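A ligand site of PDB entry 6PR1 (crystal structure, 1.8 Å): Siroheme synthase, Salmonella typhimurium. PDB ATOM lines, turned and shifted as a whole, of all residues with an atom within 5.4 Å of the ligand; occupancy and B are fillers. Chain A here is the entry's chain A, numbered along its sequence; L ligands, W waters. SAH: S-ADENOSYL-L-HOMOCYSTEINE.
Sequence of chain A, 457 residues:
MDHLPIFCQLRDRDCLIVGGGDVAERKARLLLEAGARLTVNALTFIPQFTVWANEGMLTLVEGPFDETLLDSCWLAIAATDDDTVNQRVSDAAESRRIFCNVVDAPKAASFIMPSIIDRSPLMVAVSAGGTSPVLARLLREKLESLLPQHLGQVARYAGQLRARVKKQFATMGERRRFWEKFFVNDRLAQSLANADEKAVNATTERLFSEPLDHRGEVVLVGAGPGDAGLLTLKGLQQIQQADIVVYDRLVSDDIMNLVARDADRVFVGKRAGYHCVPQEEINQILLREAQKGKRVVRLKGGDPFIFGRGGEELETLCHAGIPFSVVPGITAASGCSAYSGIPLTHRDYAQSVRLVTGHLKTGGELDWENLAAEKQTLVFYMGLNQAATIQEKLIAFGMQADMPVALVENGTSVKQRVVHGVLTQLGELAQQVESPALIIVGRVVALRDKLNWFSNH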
ATOM      1  N   PRO A 225      21.426  -3.257   5.259  1.00  0.00           N
ATOM      2  CA  PRO A 225      21.350  -2.468   6.500  1.00  0.00           C
ATOM      3  C   PRO A 225      19.998  -2.511   7.195  1.00  0.00           C
ATOM      4  O   PRO A 225      19.878  -1.988   8.302  1.00  0.00           O
ATOM      5  CB  PRO A 225      21.698  -1.041   6.014  1.00  0.00           C
ATOM      6  CG  PRO A 225      21.273  -1.023   4.584  1.00  0.00           C
ATOM      7  CD  PRO A 225      21.354  -2.421   4.049  1.00  0.00           C
ATOM      8  N   GLY A 226      18.980  -3.116   6.596  1.00  0.00           N
ATOM      9  CA  GLY A 226      17.753  -3.303   7.354  1.00  0.00           C
ATOM     10  C   GLY A 226      16.498  -3.492   6.511  1.00  0.00           C
ATOM     11  O   GLY A 226      15.723  -4.412   6.765  1.00  0.00           O
ATOM     12  N   LEU A 250      22.074  -7.014  14.217  1.00  0.00           N
ATOM     13  CA  LEU A 250      22.019  -6.059  13.119  1.00  0.00           C
ATOM     14  C   LEU A 250      21.363  -6.625  11.870  1.00  0.00           C
ATOM     15  O   LEU A 250      21.332  -5.952  10.843  1.00  0.00           O
ATOM     16  CB  LEU A 250      23.432  -5.556  12.802  1.00  0.00           C
ATOM     17  CG  LEU A 250      23.945  -4.565  13.867  1.00  0.00           C
ATOM     18  CD1 LEU A 250      25.091  -3.724  13.365  1.00  0.00           C
ATOM     19  CD2 LEU A 250      22.820  -3.651  14.351  1.00  0.00           C
ATOM     20  N   GLY A 301      24.695  -8.377   9.192  1.00  0.00           N
ATOM     21  CA  GLY A 301      24.225  -7.049   8.826  1.00  0.00           C
ATOM     22  C   GLY A 301      25.114  -6.432   7.764  1.00  0.00           C
ATOM     23  O   GLY A 301      26.339  -6.634   7.765  1.00  0.00           O
ATOM     24  N   GLY A 302      24.502  -5.685   6.837  1.00  0.00           N
ATOM     25  CA  GLY A 302      25.272  -4.967   5.812  1.00  0.00           C
ATOM     26  C   GLY A 302      25.949  -5.907   4.826  1.00  0.00           C
ATOM     27  O   GLY A 302      25.329  -6.815   4.270  1.00  0.00           O
ATOM     28  N   ASP A 303      27.264  -5.696   4.607  1.00  0.00           N
ATOM     29  CA  ASP A 303      28.123  -6.527   3.760  1.00  0.00           C
ATOM     30  C   ASP A 303      29.061  -7.362   4.627  1.00  0.00           C
ATOM     31  O   ASP A 303      29.571  -6.859   5.628  1.00  0.00           O
ATOM     32  CB  ASP A 303      28.948  -5.647   2.806  1.00  0.00           C
ATOM     33  CG  ASP A 303      29.857  -6.467   1.901  1.00  0.00           C
ATOM     34  OD1 ASP A 303      29.371  -7.026   0.892  1.00  0.00           O
ATOM     35  OD2 ASP A 303      31.063  -6.586   2.221  1.00  0.00           O
ATOM     36  N   PRO A 304      29.305  -8.652   4.300  1.00  0.00           N
ATOM     37  CA  PRO A 304      30.083  -9.503   5.211  1.00  0.00           C
ATOM     38  C   PRO A 304      31.550  -9.119   5.356  1.00  0.00           C
ATOM     39  O   PRO A 304      32.180  -9.487   6.351  1.00  0.00           O
ATOM     40  CB  PRO A 304      29.969 -10.911   4.576  1.00  0.00           C
ATOM     41  CG  PRO A 304      28.812 -10.844   3.658  1.00  0.00           C
ATOM     42  CD  PRO A 304      28.791  -9.405   3.149  1.00  0.00           C
ATOM     43  N   ILE A 306      33.003  -5.953   5.203  1.00  0.00           N
ATOM     44  CA  ILE A 306      33.256  -4.560   5.617  1.00  0.00           C
ATOM     45  C   ILE A 306      32.936  -4.463   7.117  1.00  0.00           C
ATOM     46  O   ILE A 306      31.765  -4.357   7.515  1.00  0.00           O
ATOM     47  CB  ILE A 306      32.455  -3.535   4.799  1.00  0.00           C
ATOM     48  CG1 ILE A 306      32.905  -3.563   3.335  1.00  0.00           C
ATOM     49  CG2 ILE A 306      32.651  -2.128   5.354  1.00  0.00           C
ATOM     50  CD1 ILE A 306      31.965  -2.824   2.379  1.00  0.00           C
ATOM     51  N   PHE A 307      33.982  -4.490   7.954  1.00  0.00           N
ATOM     52  CA  PHE A 307      33.856  -4.416   9.413  1.00  0.00           C
ATOM     53  C   PHE A 307      32.881  -5.457   9.946  1.00  0.00           C
ATOM     54  O   PHE A 307      32.186  -5.235  10.943  1.00  0.00           O
ATOM     55  CB  PHE A 307      33.476  -2.994   9.844  1.00  0.00           C
ATOM     56  CG  PHE A 307      34.512  -1.966   9.462  1.00  0.00           C
ATOM     57  CD1 PHE A 307      35.833  -2.125   9.850  1.00  0.00           C
ATOM     58  CD2 PHE A 307      34.167  -0.871   8.683  1.00  0.00           C
ATOM     59  CE1 PHE A 307      36.819  -1.193   9.476  1.00  0.00           C
ATOM     60  CE2 PHE A 307      35.130   0.066   8.310  1.00  0.00           C
ATOM     61  CZ  PHE A 307      36.454  -0.105   8.705  1.00  0.00           C
ATOM     62  N   GLY A 308      32.838  -6.630   9.315  1.00  0.00           N
ATOM     63  CA  GLY A 308      31.947  -7.697   9.736  1.00  0.00           C
ATOM     64  C   GLY A 308      32.610  -8.955  10.269  1.00  0.00           C
ATOM     65  O   GLY A 308      31.920  -9.902  10.658  1.00  0.00           O
ATOM     66  N   ILE A 330      24.438  -4.902   0.771  1.00  0.00           N
ATOM     67  CA  ILE A 330      24.498  -3.445   0.790  1.00  0.00           C
ATOM     68  C   ILE A 330      25.089  -3.000   2.129  1.00  0.00           C
ATOM     69  O   ILE A 330      24.486  -3.217   3.181  1.00  0.00           O
ATOM     70  CB  ILE A 330      23.107  -2.836   0.610  1.00  0.00           C
ATOM     71  CG1 ILE A 330      22.441  -3.311  -0.712  1.00  0.00           C
ATOM     72  CG2 ILE A 330      23.210  -1.319   0.696  1.00  0.00           C
ATOM     73  CD1 ILE A 330      22.999  -2.704  -1.931  1.00  0.00           C
ATOM     74  N   THR A 331      26.258  -2.366   2.091  1.00  0.00           N
ATOM     75  CA  THR A 331      26.855  -1.939   3.362  1.00  0.00           C
ATOM     76  C   THR A 331      26.111  -0.721   3.897  1.00  0.00           C
ATOM     77  O   THR A 331      25.371  -0.034   3.183  1.00  0.00           O
ATOM     78  CB  THR A 331      28.357  -1.649   3.176  1.00  0.00           C
ATOM     79  OG1 THR A 331      29.015  -1.488   4.458  1.00  0.00           O
ATOM     80  CG2 THR A 331      28.559  -0.443   2.306  1.00  0.00           C
ATOM     81  N   ALA A 332      26.273  -0.468   5.202  1.00  0.00           N
ATOM     82  CA  ALA A 332      25.501   0.614   5.813  1.00  0.00           C
ATOM     83  C   ALA A 332      25.771   1.945   5.125  1.00  0.00           C
ATOM     84  O   ALA A 332      24.856   2.765   4.996  1.00  0.00           O
ATOM     85  CB  ALA A 332      25.831   0.720   7.299  1.00  0.00           C
ATOM     86  N   ALA A 333      27.023   2.201   4.707  1.00  0.00           N
ATOM     87  CA  ALA A 333      27.334   3.460   4.021  1.00  0.00           C
ATOM     88  C   ALA A 333      26.476   3.658   2.773  1.00  0.00           C
ATOM     89  O   ALA A 333      25.976   4.756   2.537  1.00  0.00           O
ATOM     90  CB  ALA A 333      28.814   3.504   3.635  1.00  0.00           C
ATOM     91  N   CYS A 336      22.576   3.944   3.919  1.00  0.00           N
ATOM     92  CA  CYS A 336      22.306   5.208   4.593  1.00  0.00           C
ATOM     93  C   CYS A 336      22.451   6.379   3.648  1.00  0.00           C
ATOM     94  O   CYS A 336      21.689   7.353   3.724  1.00  0.00           O
ATOM     95  CB  CYS A 336      23.227   5.401   5.804  1.00  0.00           C
ATOM     96  SG  CYS A 336      22.827   4.295   7.142  1.00  0.00           S
ATOM     97  N   PHE A 380      32.002   6.972   9.424  1.00  0.00           N
ATOM     98  CA  PHE A 380      32.462   6.257  10.608  1.00  0.00           C
ATOM     99  C   PHE A 380      31.446   5.194  10.991  1.00  0.00           C
ATOM    100  O   PHE A 380      30.288   5.536  11.248  1.00  0.00           O
ATOM    101  CB  PHE A 380      32.682   7.190  11.798  1.00  0.00           C
ATOM    102  CG  PHE A 380      33.783   8.165  11.600  1.00  0.00           C
ATOM    103  CD1 PHE A 380      33.534   9.375  10.972  1.00  0.00           C
ATOM    104  CD2 PHE A 380      35.067   7.893  12.065  1.00  0.00           C
ATOM    105  CE1 PHE A 380      34.548  10.301  10.793  1.00  0.00           C
ATOM    106  CE2 PHE A 380      36.091   8.814  11.903  1.00  0.00           C
ATOM    107  CZ  PHE A 380      35.835  10.017  11.265  1.00  0.00           C
ATOM    108  N   TYR A 381      31.889   3.941  11.030  1.00  0.00           N
ATOM    109  CA  TYR A 381      31.154   2.827  11.613  1.00  0.00           C
ATOM    110  C   TYR A 381      31.461   2.687  13.101  1.00  0.00           C
ATOM    111  O   TYR A 381      32.608   2.854  13.512  1.00  0.00           O
ATOM    112  CB  TYR A 381      31.565   1.533  10.889  1.00  0.00           C
ATOM    113  CG  TYR A 381      31.036   1.391   9.485  1.00  0.00           C
ATOM    114  CD1 TYR A 381      31.439   2.262   8.458  1.00  0.00           C
ATOM    115  CD2 TYR A 381      30.154   0.365   9.160  1.00  0.00           C
ATOM    116  CE1 TYR A 381      30.946   2.115   7.140  1.00  0.00           C
ATOM    117  CE2 TYR A 381      29.659   0.225   7.857  1.00  0.00           C
ATOM    118  CZ  TYR A 381      30.067   1.089   6.861  1.00  0.00           C
ATOM    119  OH  TYR A 381      29.596   0.932   5.563  1.00  0.00           O
ATOM    120  N   MET A 382      30.445   2.310  13.897  1.00  0.00           N
ATOM    121  CA  MET A 382      30.528   2.150  15.357  1.00  0.00           C
ATOM    122  C   MET A 382      31.365   3.261  16.017  1.00  0.00           C
ATOM    123  O   MET A 382      32.289   3.011  16.799  1.00  0.00           O
ATOM    124  CB  MET A 382      31.023   0.757  15.759  1.00  0.00           C
ATOM    125  CG  MET A 382      32.233   0.225  15.012  1.00  0.00           C
ATOM    126  SD  MET A 382      32.287  -1.577  14.784  1.00  0.00           S
ATOM    127  CE  MET A 382      33.524  -1.655  13.497  1.00  0.00           C
ATOM    128  N   GLY A 383      30.982   4.504  15.718  1.00  0.00           N
ATOM    129  CA  GLY A 383      31.740   5.652  16.232  1.00  0.00           C
ATOM    130  C   GLY A 383      30.982   6.566  17.181  1.00  0.00           C
ATOM    131  O   GLY A 383      31.502   7.609  17.598  1.00  0.00           O
ATOM    132  N   VAL A 408      23.016   9.069  10.805  1.00  0.00           N
ATOM    133  CA  VAL A 408      21.879   8.323  10.306  1.00  0.00           C
ATOM    134  C   VAL A 408      21.688   7.134  11.234  1.00  0.00           C
ATOM    135  O   VAL A 408      22.575   6.277  11.319  1.00  0.00           O
ATOM    136  CB  VAL A 408      22.087   7.864   8.855  1.00  0.00           C
ATOM    137  CG1 VAL A 408      20.859   7.095   8.362  1.00  0.00           C
ATOM    138  CG2 VAL A 408      22.387   9.066   7.955  1.00  0.00           C
ATOM    139  N   GLU A 409      20.543   7.082  11.910  1.00  0.00           N
ATOM    140  CA  GLU A 409      20.231   6.046  12.882  1.00  0.00           C
ATOM    141  C   GLU A 409      19.242   5.075  12.255  1.00  0.00           C
ATOM    142  O   GLU A 409      18.221   5.492  11.721  1.00  0.00           O
ATOM    143  CB  GLU A 409      19.632   6.682  14.140  1.00  0.00           C
ATOM    144  CG  GLU A 409      19.209   5.718  15.230  1.00  0.00           C
ATOM    145  CD  GLU A 409      18.385   6.410  16.307  1.00  0.00           C
ATOM    146  OE1 GLU A 409      17.187   6.653  16.081  1.00  0.00           O
ATOM    147  OE2 GLU A 409      18.938   6.722  17.376  1.00  0.00           O
ATOM    148  N   ASN A 410      19.546   3.779  12.342  1.00  0.00           N
ATOM    149  CA  ASN A 410      18.672   2.753  11.765  1.00  0.00           C
ATOM    150  C   ASN A 410      18.371   3.076  10.298  1.00  0.00           C
ATOM    151  O   ASN A 410      17.214   3.116   9.854  1.00  0.00           O
ATOM    152  CB  ASN A 410      17.391   2.617  12.580  1.00  0.00           C
ATOM    153  CG  ASN A 410      17.609   1.830  13.858  1.00  0.00           C
ATOM    154  OD1 ASN A 410      18.160   0.727  13.818  1.00  0.00           O
ATOM    155  ND2 ASN A 410      17.216   2.397  14.983  1.00  0.00           N
ATOM    156  N   GLY A 411      19.444   3.317   9.545  1.00  0.00           N
ATOM    157  CA  GLY A 411      19.289   3.688   8.145  1.00  0.00           C
ATOM    158  C   GLY A 411      18.557   2.612   7.358  1.00  0.00           C
ATOM    159  O   GLY A 411      18.778   1.417   7.546  1.00  0.00           O
ATOM    160  N   THR A 412      17.670   3.055   6.466  1.00  0.00           N
ATOM    161  CA  THR A 412      16.840   2.282   5.536  1.00  0.00           C
ATOM    162  C   THR A 412      15.636   1.648   6.206  1.00  0.00           C
ATOM    163  O   THR A 412      14.790   1.114   5.493  1.00  0.00           O
ATOM    164  CB  THR A 412      17.597   1.175   4.760  1.00  0.00           C
ATOM    165  OG1 THR A 412      17.796   0.015   5.596  1.00  0.00           O
ATOM    166  CG2 THR A 412      18.934   1.661   4.206  1.00  0.00           C
ATOM    167  N   PRO A 436      22.049   1.250  16.067  1.00  0.00           N
ATOM    168  CA  PRO A 436      23.180   1.443  15.138  1.00  0.00           C
ATOM    169  C   PRO A 436      23.083   2.760  14.393  1.00  0.00           C
ATOM    170  O   PRO A 436      22.025   3.092  13.851  1.00  0.00           O
ATOM    171  CB  PRO A 436      23.032   0.261  14.159  1.00  0.00           C
ATOM    172  CG  PRO A 436      21.552  -0.025  14.158  1.00  0.00           C
ATOM    173  CD  PRO A 436      21.051   0.292  15.543  1.00  0.00           C
ATOM    174  N   ALA A 437      24.184   3.511  14.358  1.00  0.00           N
ATOM    175  CA  ALA A 437      24.182   4.774  13.628  1.00  0.00           C
ATOM    176  C   ALA A 437      25.510   4.952  12.908  1.00  0.00           C
ATOM    177  O   ALA A 437      26.551   4.474  13.364  1.00  0.00           O
ATOM    178  CB  ALA A 437      23.941   5.964  14.569  1.00  0.00           C
ATOM    179  N   LEU A 438      25.444   5.652  11.792  1.00  0.00           N
ATOM    180  CA  LEU A 438      26.604   6.021  10.988  1.00  0.00           C
ATOM    181  C   LEU A 438      26.847   7.517  11.122  1.00  0.00           C
ATOM    182  O   LEU A 438      25.894   8.296  11.177  1.00  0.00           O
ATOM    183  CB  LEU A 438      26.352   5.686   9.515  1.00  0.00           C
ATOM    184  CG  LEU A 438      27.362   4.928   8.659  1.00  0.00           C
ATOM    185  CD1 LEU A 438      27.852   3.660   9.316  1.00  0.00           C
ATOM    186  CD2 LEU A 438      26.707   4.664   7.318  1.00  0.00           C
HETATM  187  N   SAH L   1      29.296  -5.214   7.962  1.00  0.00           N
HETATM  188  CA  SAH L   1      28.393  -4.108   8.297  1.00  0.00           C
HETATM  189  CB  SAH L   1      28.967  -3.234   9.408  1.00  0.00           C
HETATM  190  CG  SAH L   1      28.962  -3.871  10.795  1.00  0.00           C
HETATM  191  SD  SAH L   1      29.909  -2.835  11.949  1.00  0.00           S
HETATM  192  C   SAH L   1      28.091  -3.215   7.098  1.00  0.00           C
HETATM  193  O   SAH L   1      28.623  -3.403   6.011  1.00  0.00           O
HETATM  194  OXT SAH L   1      27.317  -2.268   7.218  1.00  0.00           O
HETATM  195  C5' SAH L   1      28.409  -2.223  12.759  1.00  0.00           C
HETATM  196  C4' SAH L   1      28.196  -0.742  12.495  1.00  0.00           C
HETATM  197  O4' SAH L   1      27.582  -0.548  11.212  1.00  0.00           O
HETATM  198  C3' SAH L   1      27.216  -0.089  13.466  1.00  0.00           C
HETATM  199  O3' SAH L   1      27.817   0.275  14.692  1.00  0.00           O
HETATM  200  C2' SAH L   1      26.752   1.135  12.698  1.00  0.00           C
HETATM  201  O2' SAH L   1      27.732   2.171  12.727  1.00  0.00           O
HETATM  202  C1' SAH L   1      26.719   0.584  11.286  1.00  0.00           C
HETATM  203  N9  SAH L   1      25.375   0.194  10.849  1.00  0.00           N
HETATM  204  C8  SAH L   1      24.921  -1.080  10.569  1.00  0.00           C
HETATM  205  N7  SAH L   1      23.626  -0.986  10.158  1.00  0.00           N
HETATM  206  C5  SAH L   1      23.260   0.332  10.181  1.00  0.00           C
HETATM  207  C6  SAH L   1      22.079   0.992   9.894  1.00  0.00           C
HETATM  208  N6  SAH L   1      20.996   0.337   9.455  1.00  0.00           N
HETATM  209  N1  SAH L   1      22.023   2.365  10.030  1.00  0.00           N
HETATM  210  C2  SAH L   1      23.118   3.082  10.459  1.00  0.00           C
HETATM  211  N3  SAH L   1      24.286   2.421  10.764  1.00  0.00           N
HETATM  212  C4  SAH L   1      24.350   1.069  10.619  1.00  0.00           C
HETATM  213  O   HOH W   1      28.336  -7.369   9.550  1.00  0.00           O
HETATM  214  O   HOH W   2      25.673  -4.152  10.345  1.00  0.00           O
HETATM  215  O   HOH W   3      26.407   2.422  16.156  1.00  0.00           O
HETATM  216  O   HOH W   4      23.078  -3.649   9.580  1.00  0.00           O
HETATM  217  O   HOH W   5      26.783  -1.534  16.397  1.00  0.00           O
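The backbone carbonyl oxygen (O) of Asp 303 is in hydrogen-bond range of a nitrogen (N) of the ligand (2.9 Å).
A nitrogen (N6) of the ligand sits at hydrogen-bond distance from the backbone carbonyl oxygen of Pro 225 (2.8 Å).
A nitrogen (N1) of the ligand is in hydrogen-bond range of the backbone NH (N) of Gly 411, at 2.8 Å.
The backbone NH of Ala 332 lies within hydrogen-bond range of an oxygen (OXT) of the ligand, at 2.9 Å.
The backbone NH (N) of Asp 303 lies within hydrogen-bond range of an oxygen (O) of the ligand (3.0 Å).
O of Ala 437 is in hydrogen-bond range of O2' of the ligand (2.7 Å).
An oxygen (O) of the ligand lies within hydrogen-bond range of the side-chain hydroxyl (OG1) of Thr 331, 2.5 Å away.
The backbone carbonyl oxygen (O) of Ile 306 lies within hydrogen-bond range of a nitrogen (N) of the ligand.
The backbone carbonyl oxygen of Gly 301 is in hydrogen-bond range of a nitrogen (N) of the ligand, 3.3 Å away.
The backbone NH (N) of Met 382 lies within hydrogen-bond range of an oxygen (O2') of the ligand, 3.0 Å away.
The backbone carbonyl oxygen of Gly 411 lies within hydrogen-bond range of a nitrogen (N6) of the ligand, 3.1 Å away.
A nitrogen (N1) of the ligand sits close to the side-chain sulfur (SG) of Cys 336 (3.6 Å).
The backbone carbonyl oxygen of Val 408 sits at hydrogen-bond distance from the backbone NH of Leu 438 (3.0 Å).
The side-chain hydroxyl (OG1) of Thr 331 is in hydrogen-bond range of the side-chain hydroxyl (OH) of Tyr 381 (2.7 Å).
The side-chain sulfur (SG) of Cys 336 lies close to the backbone carbonyl oxygen (O) of Ala 332, at 3.3 Å.
The backbone NH (N) of Ala 333 sits at hydrogen-bond distance from the side-chain hydroxyl (OH) of Tyr 381, 3.0 Å away.
N of Asn 410 sits at hydrogen-bond distance from O of Pro 436 (3.0 Å).
O of Phe 307 lies close to SD of the ligand, at 3.5 Å.
Merely in contact with the ligand: Leu 250 (3.7 Å), Gly 302 (3.6 Å), Tyr 381 (3.4 Å), Val 408 (3.4 Å), Asn 410 (3.7 Å), Pro 436 (3.6 Å) and Leu 438 (3.6 Å).
Hydrophobic or aromatic side chains within 4 Å of the ligand: Pro 225, Leu 250, Ala 332, Tyr 381, Met 382, Pro 436 and Leu 438.
Within 4 Å of the ligand: Pro 225, Leu 250, Gly 301, Gly 302, Asp 303, Ile 306, Phe 307, Thr 331, Ala 332, Cys 336, Tyr 381, Met 382, Val 408, Asn 410, Gly 411, Pro 436, Ala 437 and Leu 438.
Water W4 bridges N7 of the ligand (2.8 Å) and O of Leu 250 (3.2 Å).
Water W1 bridges the backbone carbonyl oxygen of Gly 301 (2.8 Å) and a nitrogen (N) of the ligand (2.8 Å).
Water W3 bridges an oxygen (O3') of the ligand and the backbone NH of Ala 437.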
